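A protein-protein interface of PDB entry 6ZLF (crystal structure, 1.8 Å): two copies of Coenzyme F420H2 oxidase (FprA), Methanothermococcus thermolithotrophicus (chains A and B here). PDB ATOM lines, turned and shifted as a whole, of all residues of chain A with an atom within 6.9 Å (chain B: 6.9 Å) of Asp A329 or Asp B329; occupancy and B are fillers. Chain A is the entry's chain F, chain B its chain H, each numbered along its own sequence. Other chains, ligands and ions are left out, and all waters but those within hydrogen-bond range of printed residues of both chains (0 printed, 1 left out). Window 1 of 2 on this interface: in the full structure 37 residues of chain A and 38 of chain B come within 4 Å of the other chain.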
ATOM      1  N   ASP A 265     -12.039   0.926  21.528  1.00  0.00           N
ATOM      2  CA  ASP A 265     -11.516  -0.001  20.531  1.00  0.00           C
ATOM      3  C   ASP A 265     -12.089   0.413  19.179  1.00  0.00           C
ATOM      4  O   ASP A 265     -12.998   1.243  19.116  1.00  0.00           O
ATOM      5  CB  ASP A 265     -11.822  -1.474  20.853  1.00  0.00           C
ATOM      6  CG  ASP A 265     -10.716  -2.437  20.381  1.00  0.00           C
ATOM      7  OD1 ASP A 265      -9.981  -2.087  19.440  1.00  0.00           O
ATOM      8  OD2 ASP A 265     -10.602  -3.542  20.951  1.00  0.00           O
ATOM      9  N   LEU A 294      -7.884  -0.442  23.516  1.00  0.00           N
ATOM     10  CA  LEU A 294      -8.008  -1.826  24.009  1.00  0.00           C
ATOM     11  C   LEU A 294      -7.280  -2.858  23.160  1.00  0.00           C
ATOM     12  O   LEU A 294      -6.981  -3.936  23.664  1.00  0.00           O
ATOM     13  CB  LEU A 294      -9.487  -2.238  24.171  1.00  0.00           C
ATOM     14  CG  LEU A 294     -10.228  -1.588  25.325  1.00  0.00           C
ATOM     15  CD1 LEU A 294     -11.726  -1.888  25.245  1.00  0.00           C
ATOM     16  CD2 LEU A 294      -9.670  -2.056  26.679  1.00  0.00           C
ATOM     17  N   GLU A 298      -4.189  -2.890  28.460  1.00  0.00           N
ATOM     18  CA  GLU A 298      -4.873  -3.889  29.258  1.00  0.00           C
ATOM     19  C   GLU A 298      -5.443  -3.324  30.556  1.00  0.00           C
ATOM     20  O   GLU A 298      -5.181  -2.179  30.946  1.00  0.00           O
ATOM     21  CB  GLU A 298      -3.980  -5.122  29.477  1.00  0.00           C
ATOM     22  CG  GLU A 298      -2.624  -4.825  30.075  1.00  0.00           C
ATOM     23  CD  GLU A 298      -2.711  -4.306  31.494  1.00  0.00           C
ATOM     24  OE1 GLU A 298      -2.254  -3.167  31.742  1.00  0.00           O
ATOM     25  OE2 GLU A 298      -3.288  -5.020  32.349  1.00  0.00           O
ATOM     26  N   ARG A 299      -6.366  -4.096  31.119  1.00  0.00           N
ATOM     27  CA  ARG A 299      -7.260  -3.650  32.173  1.00  0.00           C
ATOM     28  C   ARG A 299      -6.568  -3.080  33.407  1.00  0.00           C
ATOM     29  O   ARG A 299      -7.118  -2.172  34.013  1.00  0.00           O
ATOM     30  CB  ARG A 299      -8.234  -4.781  32.560  1.00  0.00           C
ATOM     31  CG  ARG A 299      -7.619  -5.939  33.355  1.00  0.00           C
ATOM     32  CD  ARG A 299      -8.651  -7.023  33.605  1.00  0.00           C
ATOM     33  NE  ARG A 299      -8.751  -7.959  32.484  1.00  0.00           N
ATOM     34  CZ  ARG A 299      -7.974  -9.022  32.310  1.00  0.00           C
ATOM     35  NH1 ARG A 299      -8.173  -9.837  31.282  1.00  0.00           N
ATOM     36  NH2 ARG A 299      -6.983  -9.275  33.154  1.00  0.00           N
ATOM     37  N   PHE A 324     -18.125  -3.753  20.196  1.00  0.00           N
ATOM     38  CA  PHE A 324     -16.941  -4.569  19.895  1.00  0.00           C
ATOM     39  C   PHE A 324     -16.533  -5.388  21.138  1.00  0.00           C
ATOM     40  O   PHE A 324     -16.553  -4.851  22.242  1.00  0.00           O
ATOM     41  CB  PHE A 324     -15.790  -3.674  19.412  1.00  0.00           C
ATOM     42  CG  PHE A 324     -14.668  -4.466  18.794  1.00  0.00           C
ATOM     43  CD1 PHE A 324     -14.764  -4.937  17.492  1.00  0.00           C
ATOM     44  CD2 PHE A 324     -13.577  -4.854  19.552  1.00  0.00           C
ATOM     45  CE1 PHE A 324     -13.786  -5.785  16.966  1.00  0.00           C
ATOM     46  CE2 PHE A 324     -12.588  -5.674  19.015  1.00  0.00           C
ATOM     47  CZ  PHE A 324     -12.697  -6.129  17.726  1.00  0.00           C
ATOM     48  N   PRO A 325     -16.286  -6.710  21.004  1.00  0.00           N
ATOM     49  CA  PRO A 325     -16.240  -7.575  22.198  1.00  0.00           C
ATOM     50  C   PRO A 325     -15.141  -7.313  23.216  1.00  0.00           C
ATOM     51  O   PRO A 325     -15.309  -7.695  24.370  1.00  0.00           O
ATOM     52  CB  PRO A 325     -16.123  -8.991  21.609  1.00  0.00           C
ATOM     53  CG  PRO A 325     -15.583  -8.800  20.243  1.00  0.00           C
ATOM     54  CD  PRO A 325     -16.226  -7.519  19.772  1.00  0.00           C
ATOM     55  N   SER A 326     -14.040  -6.657  22.834  1.00  0.00           N
ATOM     56  CA  SER A 326     -12.966  -6.380  23.801  1.00  0.00           C
ATOM     57  C   SER A 326     -13.448  -5.549  25.009  1.00  0.00           C
ATOM     58  O   SER A 326     -12.899  -5.715  26.102  1.00  0.00           O
ATOM     59  CB  SER A 326     -11.811  -5.660  23.119  1.00  0.00           C
ATOM     60  OG  SER A 326     -12.299  -4.423  22.641  1.00  0.00           O
ATOM     61  N   VAL A 327     -14.513  -4.737  24.848  1.00  0.00           N
ATOM     62  CA  VAL A 327     -15.047  -3.968  25.984  1.00  0.00           C
ATOM     63  C   VAL A 327     -15.625  -4.889  27.063  1.00  0.00           C
ATOM     64  O   VAL A 327     -15.721  -4.477  28.215  1.00  0.00           O
ATOM     65  CB  VAL A 327     -16.096  -2.893  25.591  1.00  0.00           C
ATOM     66  CG1 VAL A 327     -15.548  -1.921  24.546  1.00  0.00           C
ATOM     67  CG2 VAL A 327     -17.410  -3.526  25.134  1.00  0.00           C
ATOM     68  N   GLY A 328     -16.077  -6.081  26.671  1.00  0.00           N
ATOM     69  CA  GLY A 328     -16.655  -7.047  27.598  1.00  0.00           C
ATOM     70  C   GLY A 328     -15.718  -7.424  28.724  1.00  0.00           C
ATOM     71  O   GLY A 328     -16.155  -7.594  29.862  1.00  0.00           O
ATOM     72  N   ASP A 329     -14.419  -7.556  28.418  1.00  0.00           N
ATOM     73  CA  ASP A 329     -13.411  -7.846  29.425  1.00  0.00           C
ATOM     74  C   ASP A 329     -13.347  -6.714  30.460  1.00  0.00           C
ATOM     75  O   ASP A 329     -13.438  -6.964  31.662  1.00  0.00           O
ATOM     76  CB  ASP A 329     -12.046  -8.039  28.742  1.00  0.00           C
ATOM     77  CG  ASP A 329     -10.907  -8.309  29.698  1.00  0.00           C
ATOM     78  OD1 ASP A 329     -10.674  -7.474  30.599  1.00  0.00           O
ATOM     79  OD2 ASP A 329     -10.215  -9.333  29.520  1.00  0.00           O
ATOM     80  N   LEU A 330     -13.165  -5.473  29.998  1.00  0.00           N
ATOM     81  CA  LEU A 330     -13.082  -4.341  30.921  1.00  0.00           C
ATOM     82  C   LEU A 330     -14.388  -4.173  31.725  1.00  0.00           C
ATOM     83  O   LEU A 330     -14.321  -3.916  32.924  1.00  0.00           O
ATOM     84  CB  LEU A 330     -12.751  -3.043  30.154  1.00  0.00           C
ATOM     85  CG  LEU A 330     -12.657  -1.751  31.014  1.00  0.00           C
ATOM     86  CD1 LEU A 330     -11.585  -1.862  32.089  1.00  0.00           C
ATOM     87  CD2 LEU A 330     -12.376  -0.548  30.142  1.00  0.00           C
ATOM     88  N   ILE A 331     -15.561  -4.328  31.083  1.00  0.00           N
ATOM     89  CA  ILE A 331     -16.837  -4.165  31.783  1.00  0.00           C
ATOM     90  C   ILE A 331     -16.992  -5.232  32.872  1.00  0.00           C
ATOM     91  O   ILE A 331     -17.397  -4.899  33.985  1.00  0.00           O
ATOM     92  CB  ILE A 331     -18.028  -4.147  30.788  1.00  0.00           C
ATOM     93  CG1 ILE A 331     -18.005  -2.841  29.966  1.00  0.00           C
ATOM     94  CG2 ILE A 331     -19.366  -4.301  31.523  1.00  0.00           C
ATOM     95  CD1 ILE A 331     -18.764  -2.902  28.688  1.00  0.00           C
ATOM     96  N   TYR A 332     -16.662  -6.503  32.572  1.00  0.00           N
ATOM     97  CA  TYR A 332     -16.722  -7.559  33.596  1.00  0.00           C
ATOM     98  C   TYR A 332     -15.815  -7.213  34.768  1.00  0.00           C
ATOM     99  O   TYR A 332     -16.180  -7.435  35.917  1.00  0.00           O
ATOM    100  CB  TYR A 332     -16.321  -8.926  33.024  1.00  0.00           C
ATOM    101  CG  TYR A 332     -17.488  -9.693  32.441  1.00  0.00           C
ATOM    102  CD1 TYR A 332     -18.425  -9.065  31.630  1.00  0.00           C
ATOM    103  CD2 TYR A 332     -17.634 -11.056  32.667  1.00  0.00           C
ATOM    104  CE1 TYR A 332     -19.495  -9.765  31.086  1.00  0.00           C
ATOM    105  CE2 TYR A 332     -18.720 -11.760  32.155  1.00  0.00           C
ATOM    106  CZ  TYR A 332     -19.647 -11.112  31.360  1.00  0.00           C
ATOM    107  OH  TYR A 332     -20.672 -11.822  30.782  1.00  0.00           O
ATOM    108  N   TYR A 333     -14.635  -6.661  34.481  1.00  0.00           N
ATOM    109  CA  TYR A 333     -13.704  -6.270  35.531  1.00  0.00           C
ATOM    110  C   TYR A 333     -14.261  -5.112  36.369  1.00  0.00           C
ATOM    111  O   TYR A 333     -14.190  -5.159  37.596  1.00  0.00           O
ATOM    112  CB  TYR A 333     -12.354  -5.874  34.912  1.00  0.00           C
ATOM    113  CG  TYR A 333     -11.220  -5.807  35.904  1.00  0.00           C
ATOM    114  CD1 TYR A 333     -11.064  -6.786  36.881  1.00  0.00           C
ATOM    115  CD2 TYR A 333     -10.205  -4.867  35.764  1.00  0.00           C
ATOM    116  CE1 TYR A 333      -9.967  -6.791  37.733  1.00  0.00           C
ATOM    117  CE2 TYR A 333      -9.080  -4.890  36.583  1.00  0.00           C
ATOM    118  CZ  TYR A 333      -8.949  -5.877  37.544  1.00  0.00           C
ATOM    119  OH  TYR A 333      -7.861  -5.923  38.378  1.00  0.00           O
ATOM    120  N   LEU A 334     -14.811  -4.079  35.716  1.00  0.00           N
ATOM    121  CA  LEU A 334     -15.396  -2.933  36.429  1.00  0.00           C
ATOM    122  C   LEU A 334     -16.621  -3.357  37.252  1.00  0.00           C
ATOM    123  O   LEU A 334     -16.864  -2.792  38.318  1.00  0.00           O
ATOM    124  CB  LEU A 334     -15.797  -1.823  35.440  1.00  0.00           C
ATOM    125  CG  LEU A 334     -14.644  -1.113  34.722  1.00  0.00           C
ATOM    126  CD1 LEU A 334     -15.176  -0.218  33.606  1.00  0.00           C
ATOM    127  CD2 LEU A 334     -13.800  -0.300  35.696  1.00  0.00           C
ATOM    128  N   ASP B 265     -10.191 -19.841  31.843  1.00  0.00           N
ATOM    129  CA  ASP B 265      -9.099 -19.005  32.315  1.00  0.00           C
ATOM    130  C   ASP B 265      -8.841 -19.392  33.768  1.00  0.00           C
ATOM    131  O   ASP B 265      -9.634 -20.113  34.373  1.00  0.00           O
ATOM    132  CB  ASP B 265      -9.361 -17.494  32.162  1.00  0.00           C
ATOM    133  CG  ASP B 265      -8.081 -16.694  31.871  1.00  0.00           C
ATOM    134  OD1 ASP B 265      -6.983 -17.172  32.227  1.00  0.00           O
ATOM    135  OD2 ASP B 265      -8.182 -15.599  31.278  1.00  0.00           O
ATOM    136  N   LEU B 294      -7.809 -18.863  27.776  1.00  0.00           N
ATOM    137  CA  LEU B 294      -8.027 -17.462  27.390  1.00  0.00           C
ATOM    138  C   LEU B 294      -6.829 -16.544  27.624  1.00  0.00           C
ATOM    139  O   LEU B 294      -6.759 -15.473  27.013  1.00  0.00           O
ATOM    140  CB  LEU B 294      -9.273 -16.868  28.091  1.00  0.00           C
ATOM    141  CG  LEU B 294     -10.616 -17.392  27.592  1.00  0.00           C
ATOM    142  CD1 LEU B 294     -11.749 -16.930  28.506  1.00  0.00           C
ATOM    143  CD2 LEU B 294     -10.880 -16.950  26.159  1.00  0.00           C
ATOM    144  N   GLU B 298      -7.345 -16.697  21.537  1.00  0.00           N
ATOM    145  CA  GLU B 298      -8.235 -15.591  21.239  1.00  0.00           C
ATOM    146  C   GLU B 298      -9.501 -16.034  20.520  1.00  0.00           C
ATOM    147  O   GLU B 298      -9.649 -17.190  20.105  1.00  0.00           O
ATOM    148  CB  GLU B 298      -7.487 -14.464  20.510  1.00  0.00           C
ATOM    149  CG  GLU B 298      -6.758 -14.897  19.261  1.00  0.00           C
ATOM    150  CD  GLU B 298      -7.697 -15.344  18.164  1.00  0.00           C
ATOM    151  OE1 GLU B 298      -7.601 -16.518  17.741  1.00  0.00           O
ATOM    152  OE2 GLU B 298      -8.562 -14.532  17.757  1.00  0.00           O
ATOM    153  N   ARG B 299     -10.478 -15.139  20.556  1.00  0.00           N
ATOM    154  CA  ARG B 299     -11.857 -15.441  20.227  1.00  0.00           C
ATOM    155  C   ARG B 299     -12.076 -16.049  18.838  1.00  0.00           C
ATOM    156  O   ARG B 299     -12.984 -16.869  18.700  1.00  0.00           O
ATOM    157  CB  ARG B 299     -12.736 -14.185  20.425  1.00  0.00           C
ATOM    158  CG  ARG B 299     -12.553 -13.080  19.379  1.00  0.00           C
ATOM    159  CD  ARG B 299     -13.416 -11.876  19.715  1.00  0.00           C
ATOM    160  NE  ARG B 299     -12.763 -10.961  20.650  1.00  0.00           N
ATOM    161  CZ  ARG B 299     -11.895 -10.013  20.308  1.00  0.00           C
ATOM    162  NH1 ARG B 299     -11.389  -9.203  21.229  1.00  0.00           N
ATOM    163  NH2 ARG B 299     -11.523  -9.866  19.045  1.00  0.00           N
ATOM    164  N   PHE B 324     -13.814 -14.501  36.212  1.00  0.00           N
ATOM    165  CA  PHE B 324     -12.581 -13.846  35.754  1.00  0.00           C
ATOM    166  C   PHE B 324     -12.869 -13.043  34.474  1.00  0.00           C
ATOM    167  O   PHE B 324     -13.584 -13.540  33.605  1.00  0.00           O
ATOM    168  CB  PHE B 324     -11.477 -14.889  35.525  1.00  0.00           C
ATOM    169  CG  PHE B 324     -10.117 -14.273  35.351  1.00  0.00           C
ATOM    170  CD1 PHE B 324      -9.397 -13.829  36.447  1.00  0.00           C
ATOM    171  CD2 PHE B 324      -9.628 -13.986  34.088  1.00  0.00           C
ATOM    172  CE1 PHE B 324      -8.200 -13.136  36.283  1.00  0.00           C
ATOM    173  CE2 PHE B 324      -8.419 -13.317  33.923  1.00  0.00           C
ATOM    174  CZ  PHE B 324      -7.718 -12.883  35.021  1.00  0.00           C
ATOM    175  N   PRO B 325     -12.437 -11.762  34.387  1.00  0.00           N
ATOM    176  CA  PRO B 325     -12.991 -10.869  33.355  1.00  0.00           C
ATOM    177  C   PRO B 325     -12.712 -11.214  31.899  1.00  0.00           C
ATOM    178  O   PRO B 325     -13.451 -10.754  31.040  1.00  0.00           O
ATOM    179  CB  PRO B 325     -12.398  -9.499  33.712  1.00  0.00           C
ATOM    180  CG  PRO B 325     -11.199  -9.801  34.532  1.00  0.00           C
ATOM    181  CD  PRO B 325     -11.596 -11.003  35.329  1.00  0.00           C
ATOM    182  N   SER B 326     -11.674 -12.002  31.602  1.00  0.00           N
ATOM    183  CA  SER B 326     -11.402 -12.378  30.210  1.00  0.00           C
ATOM    184  C   SER B 326     -12.579 -13.097  29.544  1.00  0.00           C
ATOM    185  O   SER B 326     -12.742 -12.976  28.330  1.00  0.00           O
ATOM    186  CB  SER B 326     -10.166 -13.263  30.138  1.00  0.00           C
ATOM    187  OG  SER B 326     -10.435 -14.451  30.863  1.00  0.00           O
ATOM    188  N   VAL B 327     -13.439 -13.785  30.317  1.00  0.00           N
ATOM    189  CA  VAL B 327     -14.612 -14.444  29.715  1.00  0.00           C
ATOM    190  C   VAL B 327     -15.576 -13.420  29.119  1.00  0.00           C
ATOM    191  O   VAL B 327     -16.333 -13.776  28.233  1.00  0.00           O
ATOM    192  CB  VAL B 327     -15.373 -15.404  30.668  1.00  0.00           C
ATOM    193  CG1 VAL B 327     -14.444 -16.473  31.248  1.00  0.00           C
ATOM    194  CG2 VAL B 327     -16.101 -14.639  31.770  1.00  0.00           C
ATOM    195  N   GLY B 328     -15.593 -12.198  29.660  1.00  0.00           N
ATOM    196  CA  GLY B 328     -16.476 -11.131  29.197  1.00  0.00           C
ATOM    197  C   GLY B 328     -16.313 -10.811  27.725  1.00  0.00           C
ATOM    198  O   GLY B 328     -17.296 -10.568  27.027  1.00  0.00           O
ATOM    199  N   ASP B 329     -15.076 -10.859  27.229  1.00  0.00           N
ATOM    200  CA  ASP B 329     -14.794 -10.645  25.818  1.00  0.00           C
ATOM    201  C   ASP B 329     -15.459 -11.738  24.975  1.00  0.00           C
ATOM    202  O   ASP B 329     -16.201 -11.437  24.037  1.00  0.00           O
ATOM    203  CB  ASP B 329     -13.267 -10.639  25.599  1.00  0.00           C
ATOM    204  CG  ASP B 329     -12.840 -10.494  24.161  1.00  0.00           C
ATOM    205  OD1 ASP B 329     -13.264 -11.323  23.329  1.00  0.00           O
ATOM    206  OD2 ASP B 329     -12.023  -9.602  23.876  1.00  0.00           O
ATOM    207  N   LEU B 330     -15.195 -13.011  25.301  1.00  0.00           N
ATOM    208  CA  LEU B 330     -15.792 -14.111  24.542  1.00  0.00           C
ATOM    209  C   LEU B 330     -17.331 -14.085  24.639  1.00  0.00           C
ATOM    210  O   LEU B 330     -17.992 -14.321  23.638  1.00  0.00           O
ATOM    211  CB  LEU B 330     -15.243 -15.463  25.030  1.00  0.00           C
ATOM    212  CG  LEU B 330     -15.812 -16.722  24.326  1.00  0.00           C
ATOM    213  CD1 LEU B 330     -15.550 -16.702  22.826  1.00  0.00           C
ATOM    214  CD2 LEU B 330     -15.226 -17.994  24.925  1.00  0.00           C
ATOM    215  N   ILE B 331     -17.899 -13.819  25.834  1.00  0.00           N
ATOM    216  CA  ILE B 331     -19.356 -13.799  25.993  1.00  0.00           C
ATOM    217  C   ILE B 331     -19.980 -12.684  25.148  1.00  0.00           C
ATOM    218  O   ILE B 331     -20.986 -12.925  24.493  1.00  0.00           O
ATOM    219  CB  ILE B 331     -19.757 -13.715  27.488  1.00  0.00           C
ATOM    220  CG1 ILE B 331     -19.426 -15.049  28.193  1.00  0.00           C
ATOM    221  CG2 ILE B 331     -21.251 -13.376  27.644  1.00  0.00           C
ATOM    222  CD1 ILE B 331     -19.311 -14.953  29.669  1.00  0.00           C
ATOM    223  N   TYR B 332     -19.382 -11.479  25.137  1.00  0.00           N
ATOM    224  CA  TYR B 332     -19.889 -10.380  24.290  1.00  0.00           C
ATOM    225  C   TYR B 332     -19.870 -10.779  22.830  1.00  0.00           C
ATOM    226  O   TYR B 332     -20.809 -10.485  22.101  1.00  0.00           O
ATOM    227  CB  TYR B 332     -19.062  -9.096  24.472  1.00  0.00           C
ATOM    228  CG  TYR B 332     -19.562  -8.212  25.592  1.00  0.00           C
ATOM    229  CD1 TYR B 332     -19.954  -8.751  26.811  1.00  0.00           C
ATOM    230  CD2 TYR B 332     -19.603  -6.830  25.449  1.00  0.00           C
ATOM    231  CE1 TYR B 332     -20.424  -7.946  27.839  1.00  0.00           C
ATOM    232  CE2 TYR B 332     -20.070  -6.012  26.473  1.00  0.00           C
ATOM    233  CZ  TYR B 332     -20.492  -6.577  27.664  1.00  0.00           C
ATOM    234  OH  TYR B 332     -20.890  -5.773  28.703  1.00  0.00           O
ATOM    235  N   TYR B 333     -18.810 -11.465  22.403  1.00  0.00           N
ATOM    236  CA  TYR B 333     -18.712 -11.956  21.034  1.00  0.00           C
ATOM    237  C   TYR B 333     -19.790 -13.018  20.747  1.00  0.00           C
ATOM    238  O   TYR B 333     -20.458 -12.937  19.722  1.00  0.00           O
ATOM    239  CB  TYR B 333     -17.305 -12.531  20.787  1.00  0.00           C
ATOM    240  CG  TYR B 333     -16.920 -12.674  19.334  1.00  0.00           C
ATOM    241  CD1 TYR B 333     -17.243 -11.691  18.407  1.00  0.00           C
ATOM    242  CD2 TYR B 333     -16.140 -13.742  18.902  1.00  0.00           C
ATOM    243  CE1 TYR B 333     -16.845 -11.791  17.080  1.00  0.00           C
ATOM    244  CE2 TYR B 333     -15.684 -13.820  17.592  1.00  0.00           C
ATOM    245  CZ  TYR B 333     -16.023 -12.829  16.688  1.00  0.00           C
ATOM    246  OH  TYR B 333     -15.635 -12.899  15.377  1.00  0.00           O
ATOM    247  N   LEU B 334     -19.970 -14.001  21.641  1.00  0.00           N
ATOM    248  CA  LEU B 334     -20.982 -15.044  21.429  1.00  0.00           C
ATOM    249  C   LEU B 334     -22.390 -14.447  21.425  1.00  0.00           C
ATOM    250  O   LEU B 334     -23.251 -14.932  20.701  1.00  0.00           O
ATOM    251  CB  LEU B 334     -20.881 -16.131  22.509  1.00  0.00           C
ATOM    252  CG  LEU B 334     -19.615 -17.002  22.472  1.00  0.00           C
ATOM    253  CD1 LEU B 334     -19.522 -17.861  23.720  1.00  0.00           C
ATOM    254  CD2 LEU B 334     -19.582 -17.871  21.219  1.00  0.00           C
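OG of Ser B326 is in hydrogen-bond range of OD2 of Asp B265 (2.6 Å). The side-chain carboxylate (OD1) of Asp B329 is in salt-bridge range of the guanidinium group (NE) of Arg B299, at 2.7 Å. The side-chain carboxylate (OD2) of Asp A265 is in hydrogen-bond range of the side-chain hydroxyl (OG) of Ser A326. The guanidinium group (NE) of Arg A299 lies within salt-bridge range of the side-chain carboxylate (OD1) of Asp A329 (2.7 Å).
NE of Arg A299 touches CG of Pro B325, at 3.7 Å. O of Pro A325 touches CA of Asp B329, at 3.3 Å. N of Tyr B333 touches CB of Pro A325 (3.7 Å). CG2 of Val A327 touches CE2 of Tyr B332 (3.9 Å). Gly A328 touches Asp B329. Tyr B332 touches Ile A331. CB of Tyr A332 touches CA of Pro B325, 3.9 Å away. CG2 of Val B327 touches CE2 of Tyr A332, 3.9 Å away. Tyr A332 touches Ile B331. CB of Pro B325 touches N of Tyr A333 (3.7 Å).
Leu A294 touches none of the printed residues of chain B. Phe A324 touches none of the printed residues of chain B. Printed residues of chain B within 4 Å of Ser A326: Asp B329. Of chain B, only Gly B328, Asp B329 and Tyr B332 come within 4 Å of Gly A328. Printed residues of chain B within 4 Å of Asp A329: Pro B325 (3.3 Å), Ser B326 (3.3 Å), Gly B328 (3.8 Å) and Asp B329 (3.6 Å). Printed residues of chain A within 4 Å of Pro B325: Arg A299, Asp A329, Tyr A332 and Tyr A333. Of the printed residues of chain A, Ser B326 touches Asp A329. Of chain A, only Gly A328 (3.6 Å), Asp A329 (3.8 Å) and Tyr A332 (3.7 Å) come within 4 Å of Gly B328. Asp B329 touches four residues of chain A. Of the printed residues of chain A, Tyr B333 touches Pro A325. The nearest residue of chain B that does not touch Asp A329 is Val B327 (5.6 Å).
Hydrophobic or aromatic side chains of chain B that line the printed part of chain A: Pro B325, Val B327, Ile B331, Tyr B332 and Tyr B333. Of the 15 printed residues of chain A, 9 touch a printed residue of chain B.
Pro A325 touches Asp B329, and with the chains exchanged Asp A329 touches Pro B325. Pro A325 touches Tyr B332, and with the chains exchanged Tyr A332 touches Pro B325. Gly A328 touches Asp B329, and with the chains exchanged Asp A329 touches Gly B328. Asp A329 touches its own counterpart, Asp B329. Of the 21 pairs that touch across the chains among the printed residues, 21 have their exchanged pair printed and touching as well.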
